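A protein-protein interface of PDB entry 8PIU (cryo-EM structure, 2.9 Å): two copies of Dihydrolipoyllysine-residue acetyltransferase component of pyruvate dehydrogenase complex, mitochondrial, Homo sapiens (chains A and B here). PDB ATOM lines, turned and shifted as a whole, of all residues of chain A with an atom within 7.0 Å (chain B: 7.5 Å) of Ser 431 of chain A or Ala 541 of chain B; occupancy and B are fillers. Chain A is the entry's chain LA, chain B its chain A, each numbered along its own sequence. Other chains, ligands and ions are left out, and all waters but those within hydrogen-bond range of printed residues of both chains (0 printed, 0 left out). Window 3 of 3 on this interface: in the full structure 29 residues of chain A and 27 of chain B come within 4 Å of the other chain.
The side-chain hydroxyl (OH) of Tyr 361 of chain B sits at hydrogen-bond distance from the backbone carbonyl oxygen (O) of Asp 539 of chain B (2.7 Å).
Among the printed residues, pairs that only touch across the chains: Ser 431 of chain A with Ala 541 of chain B, Gly 435 of chain A with Asp 539 of chain B, Leu 483 of chain A with Leu 363 of chain B, Phe 486 of chain A with Ala 541 of chain B and Phe 486 of chain A with Ala 544 of chain B.
Ser 431 of chain A touches just one residue of chain B: Ala 541. Asn 482 of chain A touches none of the printed residues of chain B. Printed residues of chain B within 4 Å of Phe 486 of chain A: Ala 541 (3.9 Å) and Ala 544 (3.4 Å). Of the printed residues of chain A, Leu 363 of chain B touches Leu 483 (3.7 Å). Ala 541 of chain B touches just these residues of chain A: Ser 431 and Phe 486. Printed residues of chain A within 4 Å of Ala 544 of chain B: Phe 486 (3.4 Å). The nearest printed residue of chain A that does not touch Leu 363 of chain B is Phe 486 of chain A (7.7 Å).
Printed residues of chain B that touch a printed residue of chain A: Leu 363, Asp 539, Ala 541 and Ala 544. Hydrophobic or aromatic side chains of chain B that line the printed part of chain A: Leu 363, Ala 541 and Ala 544. Along chain B the printed residues that touch a printed residue of chain A span positions 363 to 544. Of the 15 printed residues of chain A, 4 touch a printed residue of chain B. Hydrophobic or aromatic side chains of chain A within 4 Å of the printed part of chain B: Leu 483 and Phe 486. Among the printed residues, no Asp or Glu carboxylate lies within 4 Å of a Lys or Arg side-chain nitrogen of the other chain.
No position is printed for both chains.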
ATOM      1  N   ALA A 429     -23.141  18.823 -11.507  1.00  0.00           N
ATOM      2  CA  ALA A 429     -22.454  19.997 -12.025  1.00  0.00           C
ATOM      3  C   ALA A 429     -21.331  20.380 -11.070  1.00  0.00           C
ATOM      4  O   ALA A 429     -21.583  20.697  -9.902  1.00  0.00           O
ATOM      5  CB  ALA A 429     -23.424  21.164 -12.209  1.00  0.00           C
ATOM      6  N   VAL A 430     -20.098  20.349 -11.569  1.00  0.00           N
ATOM      7  CA  VAL A 430     -18.916  20.729 -10.808  1.00  0.00           C
ATOM      8  C   VAL A 430     -18.313  21.966 -11.455  1.00  0.00           C
ATOM      9  O   VAL A 430     -18.103  21.999 -12.675  1.00  0.00           O
ATOM     10  CB  VAL A 430     -17.886  19.586 -10.741  1.00  0.00           C
ATOM     11  CG1 VAL A 430     -16.644  20.030  -9.984  1.00  0.00           C
ATOM     12  CG2 VAL A 430     -18.497  18.357 -10.092  1.00  0.00           C
ATOM     13  N   SER A 431     -18.045  22.985 -10.638  1.00  0.00           N
ATOM     14  CA  SER A 431     -17.528  24.263 -11.121  1.00  0.00           C
ATOM     15  C   SER A 431     -16.005  24.198 -11.164  1.00  0.00           C
ATOM     16  O   SER A 431     -15.296  24.735 -10.310  1.00  0.00           O
ATOM     17  CB  SER A 431     -18.025  25.403 -10.243  1.00  0.00           C
ATOM     18  OG  SER A 431     -19.442  25.427 -10.203  1.00  0.00           O
ATOM     19  N   THR A 432     -15.501  23.514 -12.185  1.00  0.00           N
ATOM     20  CA  THR A 432     -14.068  23.487 -12.433  1.00  0.00           C
ATOM     21  C   THR A 432     -13.591  24.884 -12.827  1.00  0.00           C
ATOM     22  O   THR A 432     -14.267  25.577 -13.594  1.00  0.00           O
ATOM     23  CB  THR A 432     -13.745  22.485 -13.544  1.00  0.00           C
ATOM     24  OG1 THR A 432     -14.203  21.182 -13.160  1.00  0.00           O
ATOM     25  CG2 THR A 432     -12.250  22.426 -13.816  1.00  0.00           C
ATOM     26  N   PRO A 433     -12.422  25.326 -12.334  1.00  0.00           N
ATOM     27  CA  PRO A 433     -11.963  26.682 -12.670  1.00  0.00           C
ATOM     28  C   PRO A 433     -11.502  26.803 -14.114  1.00  0.00           C
ATOM     29  O   PRO A 433     -10.453  27.385 -14.407  1.00  0.00           O
ATOM     30  CB  PRO A 433     -10.803  26.912 -11.693  1.00  0.00           C
ATOM     31  CG  PRO A 433     -11.036  25.943 -10.581  1.00  0.00           C
ATOM     32  CD  PRO A 433     -11.645  24.740 -11.230  1.00  0.00           C
ATOM     33  N   ALA A 434     -12.302  26.245 -15.022  1.00  0.00           N
ATOM     34  CA  ALA A 434     -12.184  26.496 -16.450  1.00  0.00           C
ATOM     35  C   ALA A 434     -13.560  26.584 -17.094  1.00  0.00           C
ATOM     36  O   ALA A 434     -13.652  26.638 -18.328  1.00  0.00           O
ATOM     37  CB  ALA A 434     -11.349  25.408 -17.135  1.00  0.00           C
ATOM     38  N   GLY A 435     -14.626  26.597 -16.297  1.00  0.00           N
ATOM     39  CA  GLY A 435     -15.985  26.553 -16.797  1.00  0.00           C
ATOM     40  C   GLY A 435     -16.864  25.684 -15.921  1.00  0.00           C
ATOM     41  O   GLY A 435     -16.876  25.837 -14.697  1.00  0.00           O
ATOM     42  N   LEU A 436     -17.604  24.767 -16.536  1.00  0.00           N
ATOM     43  CA  LEU A 436     -18.436  23.820 -15.814  1.00  0.00           C
ATOM     44  C   LEU A 436     -18.238  22.433 -16.406  1.00  0.00           C
ATOM     45  O   LEU A 436     -18.020  22.284 -17.612  1.00  0.00           O
ATOM     46  CB  LEU A 436     -19.919  24.211 -15.879  1.00  0.00           C
ATOM     47  CG  LEU A 436     -20.896  23.397 -15.031  1.00  0.00           C
ATOM     48  CD1 LEU A 436     -20.743  23.739 -13.561  1.00  0.00           C
ATOM     49  CD2 LEU A 436     -22.326  23.620 -15.493  1.00  0.00           C
ATOM     50  N   ILE A 437     -18.313  21.416 -15.552  1.00  0.00           N
ATOM     51  CA  ILE A 437     -18.210  20.033 -15.995  1.00  0.00           C
ATOM     52  C   ILE A 437     -19.376  19.259 -15.398  1.00  0.00           C
ATOM     53  O   ILE A 437     -19.923  19.633 -14.357  1.00  0.00           O
ATOM     54  CB  ILE A 437     -16.850  19.408 -15.605  1.00  0.00           C
ATOM     55  CG1 ILE A 437     -16.643  18.062 -16.305  1.00  0.00           C
ATOM     56  CG2 ILE A 437     -16.747  19.260 -14.102  1.00  0.00           C
ATOM     57  CD1 ILE A 437     -16.760  18.132 -17.810  1.00  0.00           C
ATOM     58  N   ARG A 464     -11.148  18.043 -12.905  1.00  0.00           N
ATOM     59  CA  ARG A 464     -10.180  19.099 -12.629  1.00  0.00           C
ATOM     60  C   ARG A 464      -8.850  18.827 -13.318  1.00  0.00           C
ATOM     61  O   ARG A 464      -8.146  19.772 -13.695  1.00  0.00           O
ATOM     62  CB  ARG A 464      -9.987  19.262 -11.122  1.00  0.00           C
ATOM     63  CG  ARG A 464     -11.192  19.857 -10.413  1.00  0.00           C
ATOM     64  CD  ARG A 464     -10.839  20.308  -9.005  1.00  0.00           C
ATOM     65  NE  ARG A 464     -10.439  19.194  -8.154  1.00  0.00           N
ATOM     66  CZ  ARG A 464     -11.260  18.533  -7.351  1.00  0.00           C
ATOM     67  NH1 ARG A 464     -12.542  18.851  -7.261  1.00  0.00           N
ATOM     68  NH2 ARG A 464     -10.785  17.530  -6.619  1.00  0.00           N
ATOM     69  N   SER A 481     -27.342  20.607  -9.751  1.00  0.00           N
ATOM     70  CA  SER A 481     -26.378  21.694  -9.641  1.00  0.00           C
ATOM     71  C   SER A 481     -26.458  22.259  -8.232  1.00  0.00           C
ATOM     72  O   SER A 481     -27.550  22.576  -7.754  1.00  0.00           O
ATOM     73  CB  SER A 481     -26.655  22.784 -10.677  1.00  0.00           C
ATOM     74  OG  SER A 481     -25.786  23.886 -10.505  1.00  0.00           O
ATOM     75  N   ASN A 482     -25.311  22.382  -7.575  1.00  0.00           N
ATOM     76  CA  ASN A 482     -25.230  22.878  -6.208  1.00  0.00           C
ATOM     77  C   ASN A 482     -24.376  24.137  -6.184  1.00  0.00           C
ATOM     78  O   ASN A 482     -23.295  24.167  -6.779  1.00  0.00           O
ATOM     79  CB  ASN A 482     -24.641  21.811  -5.282  1.00  0.00           C
ATOM     80  CG  ASN A 482     -24.830  22.133  -3.816  1.00  0.00           C
ATOM     81  OD1 ASN A 482     -24.877  23.294  -3.421  1.00  0.00           O
ATOM     82  ND2 ASN A 482     -24.938  21.098  -2.997  1.00  0.00           N
ATOM     83  N   LEU A 483     -24.865  25.178  -5.507  1.00  0.00           N
ATOM     84  CA  LEU A 483     -24.117  26.422  -5.360  1.00  0.00           C
ATOM     85  C   LEU A 483     -24.176  26.928  -3.928  1.00  0.00           C
ATOM     86  O   LEU A 483     -24.065  28.128  -3.684  1.00  0.00           O
ATOM     87  CB  LEU A 483     -24.628  27.495  -6.322  1.00  0.00           C
ATOM     88  CG  LEU A 483     -24.304  27.333  -7.807  1.00  0.00           C
ATOM     89  CD1 LEU A 483     -24.880  28.480  -8.604  1.00  0.00           C
ATOM     90  CD2 LEU A 483     -22.808  27.242  -8.020  1.00  0.00           C
ATOM     91  N   MET A 485     -21.978  26.334  -1.596  1.00  0.00           N
ATOM     92  CA  MET A 485     -20.652  26.706  -1.120  1.00  0.00           C
ATOM     93  C   MET A 485     -20.375  28.190  -1.307  1.00  0.00           C
ATOM     94  O   MET A 485     -19.517  28.741  -0.609  1.00  0.00           O
ATOM     95  CB  MET A 485     -19.578  25.898  -1.844  1.00  0.00           C
ATOM     96  CG  MET A 485     -20.064  24.597  -2.442  1.00  0.00           C
ATOM     97  SD  MET A 485     -20.956  24.834  -3.984  1.00  0.00           S
ATOM     98  CE  MET A 485     -21.111  23.142  -4.538  1.00  0.00           C
ATOM     99  N   PHE A 486     -21.073  28.839  -2.230  1.00  0.00           N
ATOM    100  CA  PHE A 486     -20.862  30.241  -2.543  1.00  0.00           C
ATOM    101  C   PHE A 486     -21.820  31.165  -1.807  1.00  0.00           C
ATOM    102  O   PHE A 486     -21.807  32.373  -2.059  1.00  0.00           O
ATOM    103  CB  PHE A 486     -20.995  30.462  -4.047  1.00  0.00           C
ATOM    104  CG  PHE A 486     -20.111  29.572  -4.871  1.00  0.00           C
ATOM    105  CD1 PHE A 486     -18.850  29.991  -5.253  1.00  0.00           C
ATOM    106  CD2 PHE A 486     -20.544  28.320  -5.269  1.00  0.00           C
ATOM    107  CE1 PHE A 486     -18.035  29.176  -6.010  1.00  0.00           C
ATOM    108  CE2 PHE A 486     -19.735  27.500  -6.027  1.00  0.00           C
ATOM    109  CZ  PHE A 486     -18.479  27.928  -6.398  1.00  0.00           C
ATOM    110  N   TYR B 361     -30.614  33.215 -16.427  1.00  0.00           N
ATOM    111  CA  TYR B 361     -30.704  32.366 -15.247  1.00  0.00           C
ATOM    112  C   TYR B 361     -30.513  33.235 -14.014  1.00  0.00           C
ATOM    113  O   TYR B 361     -29.717  34.173 -14.025  1.00  0.00           O
ATOM    114  CB  TYR B 361     -29.693  31.212 -15.287  1.00  0.00           C
ATOM    115  CG  TYR B 361     -28.277  31.595 -14.967  1.00  0.00           C
ATOM    116  CD1 TYR B 361     -27.438  32.089 -15.949  1.00  0.00           C
ATOM    117  CD2 TYR B 361     -27.771  31.443 -13.686  1.00  0.00           C
ATOM    118  CE1 TYR B 361     -26.140  32.435 -15.664  1.00  0.00           C
ATOM    119  CE2 TYR B 361     -26.476  31.789 -13.390  1.00  0.00           C
ATOM    120  CZ  TYR B 361     -25.665  32.286 -14.385  1.00  0.00           C
ATOM    121  OH  TYR B 361     -24.370  32.634 -14.101  1.00  0.00           O
ATOM    122  N   LEU B 363     -30.064  34.167  -9.862  1.00  0.00           N
ATOM    123  CA  LEU B 363     -29.362  33.829  -8.628  1.00  0.00           C
ATOM    124  C   LEU B 363     -29.786  34.809  -7.548  1.00  0.00           C
ATOM    125  O   LEU B 363     -29.668  36.018  -7.736  1.00  0.00           O
ATOM    126  CB  LEU B 363     -27.845  33.891  -8.822  1.00  0.00           C
ATOM    127  CG  LEU B 363     -27.165  32.956  -9.816  1.00  0.00           C
ATOM    128  CD1 LEU B 363     -26.038  33.685 -10.503  1.00  0.00           C
ATOM    129  CD2 LEU B 363     -26.636  31.738  -9.099  1.00  0.00           C
ATOM    130  N   VAL B 406     -15.109  41.286 -10.286  1.00  0.00           N
ATOM    131  CA  VAL B 406     -15.478  40.193 -11.187  1.00  0.00           C
ATOM    132  C   VAL B 406     -15.868  40.782 -12.538  1.00  0.00           C
ATOM    133  O   VAL B 406     -17.013  41.221 -12.721  1.00  0.00           O
ATOM    134  CB  VAL B 406     -16.612  39.337 -10.603  1.00  0.00           C
ATOM    135  CG1 VAL B 406     -17.028  38.272 -11.594  1.00  0.00           C
ATOM    136  CG2 VAL B 406     -16.173  38.687  -9.312  1.00  0.00           C
ATOM    137  N   HIS B 535     -26.123  33.137 -19.341  1.00  0.00           N
ATOM    138  CA  HIS B 535     -25.337  31.946 -19.045  1.00  0.00           C
ATOM    139  C   HIS B 535     -24.255  31.679 -20.082  1.00  0.00           C
ATOM    140  O   HIS B 535     -23.303  30.949 -19.788  1.00  0.00           O
ATOM    141  CB  HIS B 535     -26.252  30.731 -18.922  1.00  0.00           C
ATOM    142  CG  HIS B 535     -25.699  29.647 -18.049  1.00  0.00           C
ATOM    143  ND1 HIS B 535     -26.375  28.473 -17.802  1.00  0.00           N
ATOM    144  CD2 HIS B 535     -24.536  29.563 -17.362  1.00  0.00           C
ATOM    145  CE1 HIS B 535     -25.651  27.711 -17.002  1.00  0.00           C
ATOM    146  NE2 HIS B 535     -24.531  28.349 -16.719  1.00  0.00           N
ATOM    147  N   VAL B 538     -21.800  34.548 -18.344  1.00  0.00           N
ATOM    148  CA  VAL B 538     -21.571  34.442 -16.909  1.00  0.00           C
ATOM    149  C   VAL B 538     -21.919  33.028 -16.466  1.00  0.00           C
ATOM    150  O   VAL B 538     -23.034  32.550 -16.710  1.00  0.00           O
ATOM    151  CB  VAL B 538     -22.394  35.476 -16.127  1.00  0.00           C
ATOM    152  CG1 VAL B 538     -22.043  35.426 -14.651  1.00  0.00           C
ATOM    153  CG2 VAL B 538     -22.172  36.865 -16.688  1.00  0.00           C
ATOM    154  N   ASP B 539     -20.970  32.361 -15.817  1.00  0.00           N
ATOM    155  CA  ASP B 539     -21.223  31.058 -15.226  1.00  0.00           C
ATOM    156  C   ASP B 539     -21.862  31.218 -13.849  1.00  0.00           C
ATOM    157  O   ASP B 539     -21.875  32.302 -13.259  1.00  0.00           O
ATOM    158  CB  ASP B 539     -19.929  30.254 -15.119  1.00  0.00           C
ATOM    159  CG  ASP B 539     -19.245  30.072 -16.458  1.00  0.00           C
ATOM    160  OD1 ASP B 539     -19.742  30.629 -17.460  1.00  0.00           O
ATOM    161  OD2 ASP B 539     -18.212  29.372 -16.508  1.00  0.00           O
ATOM    162  N   GLY B 540     -22.414  30.115 -13.341  1.00  0.00           N
ATOM    163  CA  GLY B 540     -23.057  30.159 -12.039  1.00  0.00           C
ATOM    164  C   GLY B 540     -22.094  30.513 -10.924  1.00  0.00           C
ATOM    165  O   GLY B 540     -22.416  31.314 -10.044  1.00  0.00           O
ATOM    166  N   ALA B 541     -20.894  29.928 -10.951  1.00  0.00           N
ATOM    167  CA  ALA B 541     -19.891  30.249  -9.940  1.00  0.00           C
ATOM    168  C   ALA B 541     -19.451  31.703 -10.042  1.00  0.00           C
ATOM    169  O   ALA B 541     -19.224  32.363  -9.022  1.00  0.00           O
ATOM    170  CB  ALA B 541     -18.693  29.312 -10.077  1.00  0.00           C
ATOM    171  N   VAL B 542     -19.324  32.219 -11.266  1.00  0.00           N
ATOM    172  CA  VAL B 542     -18.935  33.613 -11.460  1.00  0.00           C
ATOM    173  C   VAL B 542     -19.991  34.550 -10.883  1.00  0.00           C
ATOM    174  O   VAL B 542     -19.677  35.501 -10.155  1.00  0.00           O
ATOM    175  CB  VAL B 542     -18.689  33.888 -12.953  1.00  0.00           C
ATOM    176  CG1 VAL B 542     -18.404  35.353 -13.186  1.00  0.00           C
ATOM    177  CG2 VAL B 542     -17.548  33.032 -13.462  1.00  0.00           C
ATOM    178  N   GLY B 543     -21.263  34.292 -11.200  1.00  0.00           N
ATOM    179  CA  GLY B 543     -22.329  35.110 -10.647  1.00  0.00           C
ATOM    180  C   GLY B 543     -22.412  35.013  -9.137  1.00  0.00           C
ATOM    181  O   GLY B 543     -22.698  36.000  -8.452  1.00  0.00           O
ATOM    182  N   ALA B 544     -22.156  33.825  -8.596  1.00  0.00           N
ATOM    183  CA  ALA B 544     -22.168  33.651  -7.150  1.00  0.00           C
ATOM    184  C   ALA B 544     -21.038  34.429  -6.486  1.00  0.00           C
ATOM    185  O   ALA B 544     -21.229  35.014  -5.415  1.00  0.00           O
ATOM    186  CB  ALA B 544     -22.083  32.166  -6.815  1.00  0.00           C
ATOM    187  N   GLN B 545     -19.853  34.444  -7.103  1.00  0.00           N
ATOM    188  CA  GLN B 545     -18.756  35.259  -6.588  1.00  0.00           C
ATOM    189  C   GLN B 545     -19.102  36.740  -6.631  1.00  0.00           C
ATOM    190  O   GLN B 545     -18.796  37.489  -5.692  1.00  0.00           O
ATOM    191  CB  GLN B 545     -17.481  34.996  -7.386  1.00  0.00           C
ATOM    192  CG  GLN B 545     -16.912  33.602  -7.228  1.00  0.00           C
ATOM    193  CD  GLN B 545     -15.806  33.314  -8.224  1.00  0.00           C
ATOM    194  OE1 GLN B 545     -15.250  34.229  -8.832  1.00  0.00           O
ATOM    195  NE2 GLN B 545     -15.486  32.038  -8.401  1.00  0.00           N
ATOM    196  N   TRP B 546     -19.722  37.184  -7.726  1.00  0.00           N
ATOM    197  CA  TRP B 546     -20.135  38.579  -7.825  1.00  0.00           C
ATOM    198  C   TRP B 546     -21.100  38.938  -6.703  1.00  0.00           C
ATOM    199  O   TRP B 546     -20.972  39.990  -6.066  1.00  0.00           O
ATOM    200  CB  TRP B 546     -20.772  38.834  -9.190  1.00  0.00           C
ATOM    201  CG  TRP B 546     -21.015  40.280  -9.497  1.00  0.00           C
ATOM    202  CD1 TRP B 546     -20.248  41.086 -10.277  1.00  0.00           C
ATOM    203  CD2 TRP B 546     -22.105  41.090  -9.035  1.00  0.00           C
ATOM    204  NE1 TRP B 546     -20.787  42.344 -10.333  1.00  0.00           N
ATOM    205  CE2 TRP B 546     -21.927  42.374  -9.577  1.00  0.00           C
ATOM    206  CE3 TRP B 546     -23.214  40.853  -8.218  1.00  0.00           C
ATOM    207  CZ2 TRP B 546     -22.809  43.417  -9.324  1.00  0.00           C
ATOM    208  CZ3 TRP B 546     -24.087  41.889  -7.968  1.00  0.00           C
ATOM    209  CH2 TRP B 546     -23.881  43.155  -8.520  1.00  0.00           C
ATOM    210  N   LEU B 547     -22.074  38.065  -6.444  1.00  0.00           N
ATOM    211  CA  LEU B 547     -23.026  38.322  -5.369  1.00  0.00           C
ATOM    212  C   LEU B 547     -22.345  38.316  -4.007  1.00  0.00           C
ATOM    213  O   LEU B 547     -22.702  39.106  -3.128  1.00  0.00           O
ATOM    214  CB  LEU B 547     -24.155  37.295  -5.413  1.00  0.00           C
ATOM    215  CG  LEU B 547     -25.207  37.486  -6.506  1.00  0.00           C
ATOM    216  CD1 LEU B 547     -26.018  36.223  -6.678  1.00  0.00           C
ATOM    217  CD2 LEU B 547     -26.116  38.652  -6.169  1.00  0.00           C
